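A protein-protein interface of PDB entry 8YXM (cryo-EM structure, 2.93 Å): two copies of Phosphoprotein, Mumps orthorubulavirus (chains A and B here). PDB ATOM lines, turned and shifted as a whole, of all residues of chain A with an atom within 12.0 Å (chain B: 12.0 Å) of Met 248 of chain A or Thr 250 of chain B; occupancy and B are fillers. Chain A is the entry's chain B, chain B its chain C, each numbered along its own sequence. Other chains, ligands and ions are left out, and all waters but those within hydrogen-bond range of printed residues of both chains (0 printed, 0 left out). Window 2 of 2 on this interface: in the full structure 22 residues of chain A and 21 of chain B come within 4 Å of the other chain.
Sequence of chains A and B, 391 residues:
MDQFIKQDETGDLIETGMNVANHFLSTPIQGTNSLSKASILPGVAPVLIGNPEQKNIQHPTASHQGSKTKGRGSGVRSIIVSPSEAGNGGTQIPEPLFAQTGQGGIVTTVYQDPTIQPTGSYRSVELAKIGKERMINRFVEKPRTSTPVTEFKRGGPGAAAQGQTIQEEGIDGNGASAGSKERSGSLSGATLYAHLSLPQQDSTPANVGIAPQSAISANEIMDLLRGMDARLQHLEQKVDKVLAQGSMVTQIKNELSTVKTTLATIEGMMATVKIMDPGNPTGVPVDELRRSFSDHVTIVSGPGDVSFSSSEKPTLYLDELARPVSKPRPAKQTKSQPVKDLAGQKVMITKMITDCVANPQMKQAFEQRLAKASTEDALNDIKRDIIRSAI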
ATOM      1  N   MET A 248      15.977  -3.217  21.208  1.00  0.00           N
ATOM      2  CA  MET A 248      17.006  -2.783  20.270  1.00  0.00           C
ATOM      3  C   MET A 248      18.151  -3.792  20.216  1.00  0.00           C
ATOM      4  O   MET A 248      18.814  -3.936  19.189  1.00  0.00           O
ATOM      5  CB  MET A 248      17.533  -1.399  20.655  1.00  0.00           C
ATOM      6  CG  MET A 248      18.222  -0.656  19.523  1.00  0.00           C
ATOM      7  SD  MET A 248      20.011  -0.569  19.735  1.00  0.00           S
ATOM      8  CE  MET A 248      20.132   0.545  21.132  1.00  0.00           C
ATOM      9  N   VAL A 249      18.377  -4.487  21.333  1.00  0.00           N
ATOM     10  CA  VAL A 249      19.404  -5.524  21.370  1.00  0.00           C
ATOM     11  C   VAL A 249      19.039  -6.668  20.431  1.00  0.00           C
ATOM     12  O   VAL A 249      19.901  -7.227  19.742  1.00  0.00           O
ATOM     13  CB  VAL A 249      19.612  -6.010  22.817  1.00  0.00           C
ATOM     14  CG1 VAL A 249      20.299  -7.368  22.841  1.00  0.00           C
ATOM     15  CG2 VAL A 249      20.416  -4.989  23.608  1.00  0.00           C
ATOM     16  N   THR A 250      17.754  -7.028  20.382  1.00  0.00           N
ATOM     17  CA  THR A 250      17.311  -8.057  19.449  1.00  0.00           C
ATOM     18  C   THR A 250      17.544  -7.627  18.006  1.00  0.00           C
ATOM     19  O   THR A 250      17.897  -8.450  17.154  1.00  0.00           O
ATOM     20  CB  THR A 250      15.834  -8.375  19.683  1.00  0.00           C
ATOM     21  OG1 THR A 250      15.037  -7.242  19.311  1.00  0.00           O
ATOM     22  CG2 THR A 250      15.589  -8.703  21.148  1.00  0.00           C
ATOM     23  N   GLN A 251      17.349  -6.339  17.713  1.00  0.00           N
ATOM     24  CA  GLN A 251      17.629  -5.831  16.374  1.00  0.00           C
ATOM     25  C   GLN A 251      19.102  -5.987  16.019  1.00  0.00           C
ATOM     26  O   GLN A 251      19.441  -6.424  14.910  1.00  0.00           O
ATOM     27  CB  GLN A 251      17.205  -4.365  16.275  1.00  0.00           C
ATOM     28  CG  GLN A 251      17.566  -3.693  14.960  1.00  0.00           C
ATOM     29  CD  GLN A 251      17.077  -2.259  14.886  1.00  0.00           C
ATOM     30  OE1 GLN A 251      16.576  -1.710  15.867  1.00  0.00           O
ATOM     31  NE2 GLN A 251      17.223  -1.644  13.718  1.00  0.00           N
ATOM     32  N   ILE A 252      19.996  -5.637  16.949  1.00  0.00           N
ATOM     33  CA  ILE A 252      21.421  -5.757  16.666  1.00  0.00           C
ATOM     34  C   ILE A 252      21.817  -7.221  16.526  1.00  0.00           C
ATOM     35  O   ILE A 252      22.687  -7.553  15.719  1.00  0.00           O
ATOM     36  CB  ILE A 252      22.260  -5.018  17.731  1.00  0.00           C
ATOM     37  CG1 ILE A 252      23.536  -4.459  17.101  1.00  0.00           C
ATOM     38  CG2 ILE A 252      22.630  -5.924  18.895  1.00  0.00           C
ATOM     39  CD1 ILE A 252      23.291  -3.318  16.139  1.00  0.00           C
ATOM     40  N   LYS A 253      21.177  -8.123  17.276  1.00  0.00           N
ATOM     41  CA  LYS A 253      21.469  -9.546  17.120  1.00  0.00           C
ATOM     42  C   LYS A 253      21.008 -10.057  15.759  1.00  0.00           C
ATOM     43  O   LYS A 253      21.739 -10.791  15.078  1.00  0.00           O
ATOM     44  CB  LYS A 253      20.813 -10.337  18.252  1.00  0.00           C
ATOM     45  CG  LYS A 253      21.154 -11.816  18.270  1.00  0.00           C
ATOM     46  CD  LYS A 253      19.961 -12.667  17.872  1.00  0.00           C
ATOM     47  CE  LYS A 253      20.267 -14.147  18.031  1.00  0.00           C
ATOM     48  NZ  LYS A 253      20.704 -14.476  19.417  1.00  0.00           N
ATOM     49  N   ASN A 254      19.803  -9.664  15.338  1.00  0.00           N
ATOM     50  CA  ASN A 254      19.294 -10.088  14.039  1.00  0.00           C
ATOM     51  C   ASN A 254      20.176  -9.572  12.910  1.00  0.00           C
ATOM     52  O   ASN A 254      20.431 -10.287  11.935  1.00  0.00           O
ATOM     53  CB  ASN A 254      17.854  -9.607  13.861  1.00  0.00           C
ATOM     54  CG  ASN A 254      17.108 -10.381  12.793  1.00  0.00           C
ATOM     55  OD1 ASN A 254      17.680 -11.233  12.113  1.00  0.00           O
ATOM     56  ND2 ASN A 254      15.822 -10.086  12.638  1.00  0.00           N
ATOM     57  N   GLU A 255      20.653  -8.330  13.023  1.00  0.00           N
ATOM     58  CA  GLU A 255      21.514  -7.778  11.983  1.00  0.00           C
ATOM     59  C   GLU A 255      22.920  -8.370  12.030  1.00  0.00           C
ATOM     60  O   GLU A 255      23.552  -8.559  10.980  1.00  0.00           O
ATOM     61  CB  GLU A 255      21.555  -6.255  12.105  1.00  0.00           C
ATOM     62  CG  GLU A 255      22.670  -5.588  11.334  1.00  0.00           C
ATOM     63  CD  GLU A 255      22.698  -4.094  11.550  1.00  0.00           C
ATOM     64  OE1 GLU A 255      21.835  -3.582  12.293  1.00  0.00           O
ATOM     65  OE2 GLU A 255      23.576  -3.429  10.967  1.00  0.00           O
ATOM     66  N   LEU A 256      23.427  -8.689  13.222  1.00  0.00           N
ATOM     67  CA  LEU A 256      24.709  -9.367  13.306  1.00  0.00           C
ATOM     68  C   LEU A 256      24.632 -10.789  12.778  1.00  0.00           C
ATOM     69  O   LEU A 256      25.662 -11.346  12.405  1.00  0.00           O
ATOM     70  CB  LEU A 256      25.229  -9.372  14.743  1.00  0.00           C
ATOM     71  CG  LEU A 256      26.754  -9.486  14.816  1.00  0.00           C
ATOM     72  CD1 LEU A 256      27.392  -8.294  14.128  1.00  0.00           C
ATOM     73  CD2 LEU A 256      27.248  -9.607  16.245  1.00  0.00           C
ATOM     74  N   SER A 257      23.442 -11.388  12.729  1.00  0.00           N
ATOM     75  CA  SER A 257      23.299 -12.658  12.020  1.00  0.00           C
ATOM     76  C   SER A 257      23.618 -12.494  10.534  1.00  0.00           C
ATOM     77  O   SER A 257      24.329 -13.316   9.936  1.00  0.00           O
ATOM     78  CB  SER A 257      21.887 -13.212  12.215  1.00  0.00           C
ATOM     79  OG  SER A 257      21.727 -14.450  11.544  1.00  0.00           O
ATOM     80  N   MET B 248      25.125   4.706  25.267  1.00  0.00           N
ATOM     81  CA  MET B 248      26.279   4.388  24.384  1.00  0.00           C
ATOM     82  C   MET B 248      25.892   3.232  23.457  1.00  0.00           C
ATOM     83  O   MET B 248      26.276   3.269  22.276  1.00  0.00           O
ATOM     84  CB  MET B 248      27.504   3.989  25.214  1.00  0.00           C
ATOM     85  CG  MET B 248      28.822   4.102  24.465  1.00  0.00           C
ATOM     86  SD  MET B 248      29.176   2.695  23.378  1.00  0.00           S
ATOM     87  CE  MET B 248      29.094   1.343  24.552  1.00  0.00           C
ATOM     88  N   VAL B 249      25.159   2.245  23.978  1.00  0.00           N
ATOM     89  CA  VAL B 249      24.775   1.094  23.163  1.00  0.00           C
ATOM     90  C   VAL B 249      24.018   1.537  21.918  1.00  0.00           C
ATOM     91  O   VAL B 249      24.019   0.838  20.898  1.00  0.00           O
ATOM     92  CB  VAL B 249      23.949   0.103  24.009  1.00  0.00           C
ATOM     93  CG1 VAL B 249      23.680  -1.179  23.235  1.00  0.00           C
ATOM     94  CG2 VAL B 249      24.663  -0.198  25.317  1.00  0.00           C
ATOM     95  N   THR B 250      23.363   2.699  21.973  1.00  0.00           N
ATOM     96  CA  THR B 250      22.733   3.239  20.774  1.00  0.00           C
ATOM     97  C   THR B 250      23.769   3.645  19.733  1.00  0.00           C
ATOM     98  O   THR B 250      23.497   3.572  18.528  1.00  0.00           O
ATOM     99  CB  THR B 250      21.843   4.430  21.132  1.00  0.00           C
ATOM    100  OG1 THR B 250      21.478   5.133  19.938  1.00  0.00           O
ATOM    101  CG2 THR B 250      22.571   5.378  22.074  1.00  0.00           C
ATOM    102  N   GLN B 251      24.955   4.075  20.171  1.00  0.00           N
ATOM    103  CA  GLN B 251      25.987   4.500  19.228  1.00  0.00           C
ATOM    104  C   GLN B 251      26.486   3.330  18.389  1.00  0.00           C
ATOM    105  O   GLN B 251      26.652   3.454  17.170  1.00  0.00           O
ATOM    106  CB  GLN B 251      27.148   5.157  19.973  1.00  0.00           C
ATOM    107  CG  GLN B 251      26.817   6.503  20.594  1.00  0.00           C
ATOM    108  CD  GLN B 251      27.937   7.025  21.472  1.00  0.00           C
ATOM    109  OE1 GLN B 251      29.046   6.491  21.466  1.00  0.00           O
ATOM    110  NE2 GLN B 251      27.653   8.074  22.235  1.00  0.00           N
ATOM    111  N   ILE B 252      26.738   2.182  19.024  1.00  0.00           N
ATOM    112  CA  ILE B 252      27.225   1.026  18.280  1.00  0.00           C
ATOM    113  C   ILE B 252      26.167   0.487  17.328  1.00  0.00           C
ATOM    114  O   ILE B 252      26.504  -0.221  16.372  1.00  0.00           O
ATOM    115  CB  ILE B 252      27.719  -0.076  19.243  1.00  0.00           C
ATOM    116  CG1 ILE B 252      26.554  -0.728  19.994  1.00  0.00           C
ATOM    117  CG2 ILE B 252      28.727   0.491  20.226  1.00  0.00           C
ATOM    118  CD1 ILE B 252      26.101  -2.061  19.421  1.00  0.00           C
ATOM    119  N   LYS B 253      24.890   0.796  17.566  1.00  0.00           N
ATOM    120  CA  LYS B 253      23.836   0.326  16.675  1.00  0.00           C
ATOM    121  C   LYS B 253      23.968   0.938  15.286  1.00  0.00           C
ATOM    122  O   LYS B 253      23.846   0.234  14.277  1.00  0.00           O
ATOM    123  CB  LYS B 253      22.466   0.637  17.278  1.00  0.00           C
ATOM    124  CG  LYS B 253      21.381   0.946  16.257  1.00  0.00           C
ATOM    125  CD  LYS B 253      20.820  -0.321  15.636  1.00  0.00           C
ATOM    126  CE  LYS B 253      20.113  -0.018  14.328  1.00  0.00           C
ATOM    127  NZ  LYS B 253      19.150   1.108  14.474  1.00  0.00           N
ATOM    128  N   ASN B 254      24.218   2.247  15.209  1.00  0.00           N
ATOM    129  CA  ASN B 254      24.341   2.890  13.904  1.00  0.00           C
ATOM    130  C   ASN B 254      25.671   2.555  13.244  1.00  0.00           C
ATOM    131  O   ASN B 254      25.728   2.340  12.028  1.00  0.00           O
ATOM    132  CB  ASN B 254      24.170   4.404  14.039  1.00  0.00           C
ATOM    133  CG  ASN B 254      24.958   4.981  15.198  1.00  0.00           C
ATOM    134  OD1 ASN B 254      24.450   5.095  16.313  1.00  0.00           O
ATOM    135  ND2 ASN B 254      26.206   5.351  14.940  1.00  0.00           N
ATOM    136  N   GLU B 255      26.753   2.506  14.028  1.00  0.00           N
ATOM    137  CA  GLU B 255      28.065   2.209  13.461  1.00  0.00           C
ATOM    138  C   GLU B 255      28.117   0.798  12.890  1.00  0.00           C
ATOM    139  O   GLU B 255      28.732   0.567  11.841  1.00  0.00           O
ATOM    140  CB  GLU B 255      29.153   2.397  14.518  1.00  0.00           C
ATOM    141  CG  GLU B 255      29.499   3.848  14.807  1.00  0.00           C
ATOM    142  CD  GLU B 255      29.455   4.172  16.285  1.00  0.00           C
ATOM    143  OE1 GLU B 255      29.622   3.242  17.104  1.00  0.00           O
ATOM    144  OE2 GLU B 255      29.253   5.355  16.632  1.00  0.00           O
ATOM    145  N   LEU B 256      27.487  -0.162  13.570  1.00  0.00           N
ATOM    146  CA  LEU B 256      27.472  -1.531  13.067  1.00  0.00           C
ATOM    147  C   LEU B 256      26.717  -1.614  11.746  1.00  0.00           C
ATOM    148  O   LEU B 256      27.071  -2.422  10.879  1.00  0.00           O
ATOM    149  CB  LEU B 256      26.869  -2.460  14.128  1.00  0.00           C
ATOM    150  CG  LEU B 256      26.794  -3.992  14.022  1.00  0.00           C
ATOM    151  CD1 LEU B 256      25.859  -4.512  12.941  1.00  0.00           C
ATOM    152  CD2 LEU B 256      28.194  -4.560  13.835  1.00  0.00           C
ATOM    153  N   SER B 257      25.687  -0.783  11.570  1.00  0.00           N
ATOM    154  CA  SER B 257      24.977  -0.744  10.295  1.00  0.00           C
ATOM    155  C   SER B 257      25.883  -0.249   9.174  1.00  0.00           C
ATOM    156  O   SER B 257      25.767  -0.702   8.030  1.00  0.00           O
ATOM    157  CB  SER B 257      23.733   0.136  10.411  1.00  0.00           C
ATOM    158  OG  SER B 257      22.879  -0.041   9.294  1.00  0.00           O
ATOM    159  N   THR B 258      26.784   0.687   9.482  1.00  0.00           N
ATOM    160  CA  THR B 258      27.777   1.100   8.497  1.00  0.00           C
ATOM    161  C   THR B 258      28.682  -0.064   8.118  1.00  0.00           C
ATOM    162  O   THR B 258      29.013  -0.245   6.941  1.00  0.00           O
ATOM    163  CB  THR B 258      28.606   2.266   9.035  1.00  0.00           C
ATOM    164  OG1 THR B 258      29.549   1.779   9.998  1.00  0.00           O
ATOM    165  CG2 THR B 258      27.708   3.305   9.688  1.00  0.00           C
ATOM    166  N   VAL B 259      29.086  -0.867   9.105  1.00  0.00           N
ATOM    167  CA  VAL B 259      29.919  -2.036   8.832  1.00  0.00           C
ATOM    168  C   VAL B 259      29.173  -3.030   7.953  1.00  0.00           C
ATOM    169  O   VAL B 259      29.739  -3.590   7.006  1.00  0.00           O
ATOM    170  CB  VAL B 259      30.380  -2.682  10.151  1.00  0.00           C
ATOM    171  CG1 VAL B 259      31.227  -3.912   9.873  1.00  0.00           C
ATOM    172  CG2 VAL B 259      31.154  -1.675  10.989  1.00  0.00           C
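The side-chain amide nitrogen of Gln 251 of chain A lies close to the side-chain amino group of Lys 253 of chain B (3.4 Å).
OE2 of Glu 255 of chain A lies close to N of Ser 257 of chain B (3.4 Å).
The side-chain amide oxygen of Asn 254 of chain B lies close to the backbone carbonyl oxygen of Thr 250 of chain B (2.9 Å).
Among the printed residues, merely in contact across the chains: Glu 255 of chain A with Leu 256 of chain B (3.2 Å), Met 248 of chain A with Lys 253 of chain B (3.7 Å), Ile 252 of chain A with Lys 253 of chain B (3.7 Å), Met 248 of chain A with Thr 250 of chain B (3.8 Å), Leu 256 of chain A with Leu 256 of chain B (3.8 Å) and Met 248 of chain A with Val 249 of chain B (3.9 Å).
Met 248 of chain A touches just these residues of chain B: Val 249, Thr 250 and Lys 253.
Of chain A, only Met 248 (3.8 Å) comes within 4 Å of Thr 250 of chain B.
No residue of chain B comes within 4 Å of Val 249 of chain A.
No residue of chain B comes within 4 Å of Thr 250 of chain A.
Of chain B, only Lys 253 (3.4 Å) comes within 4 Å of Gln 251 of chain A.
Ile 252 of chain A touches just one residue of chain B: Lys 253 (3.7 Å).
No residue of chain A comes within 4 Å of Ile 252 of chain B.
No residue of chain A comes within 4 Å of Asn 254 of chain B.
Printed residues of chain A within 4 Å of Ser 257 of chain B: Glu 255 (3.1 Å).
Of the printed residues of chain A, Leu 256 of chain B touches Glu 255 (3.2 Å) and Leu 256 (3.8 Å).
Printed residues of chain B within 4 Å of Leu 256 of chain A: Leu 256.
Printed residues of chain B within 4 Å of Glu 255 of chain A: Leu 256 (3.2 Å) and Ser 257 (3.1 Å).
Asn 254 of chain A touches none of the printed residues of chain B.
Thr 258 of chain B touches none of the printed residues of chain A.
The nearest residue of chain A that does not touch Thr 250 of chain B is Ile 252 of chain A (7.3 Å).
The nearest printed residue of chain B that does not touch Leu 256 of chain A is Val 259 of chain B (7.2 Å).
Of the 12 printed residues of chain B, 5 touch a printed residue of chain A.
Of the 10 printed residues of chain A, 5 touch a printed residue of chain B.
Hydrophobic or aromatic side chains of chain A within 4 Å of the printed part of chain B: Met 248, Ile 252 and Leu 256.
Among the printed residues, 8 pairs touch across the chains.
Met 248 of chain A touches Val 249 of chain B, but with the chains exchanged Val 249 of chain A does not touch Met 248 of chain B (9.9 Å).
Ile 252 of chain A touches Lys 253 of chain B, but with the chains exchanged Lys 253 of chain A does not touch Ile 252 of chain B (8.1 Å).
Glu 255 of chain A touches Leu 256 of chain B, but with the chains exchanged Leu 256 of chain A does not touch Glu 255 of chain B (9.2 Å).
Leu 256 of chain A touches its own counterpart, Leu 256 of chain B.
10 positions are printed for both chains.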
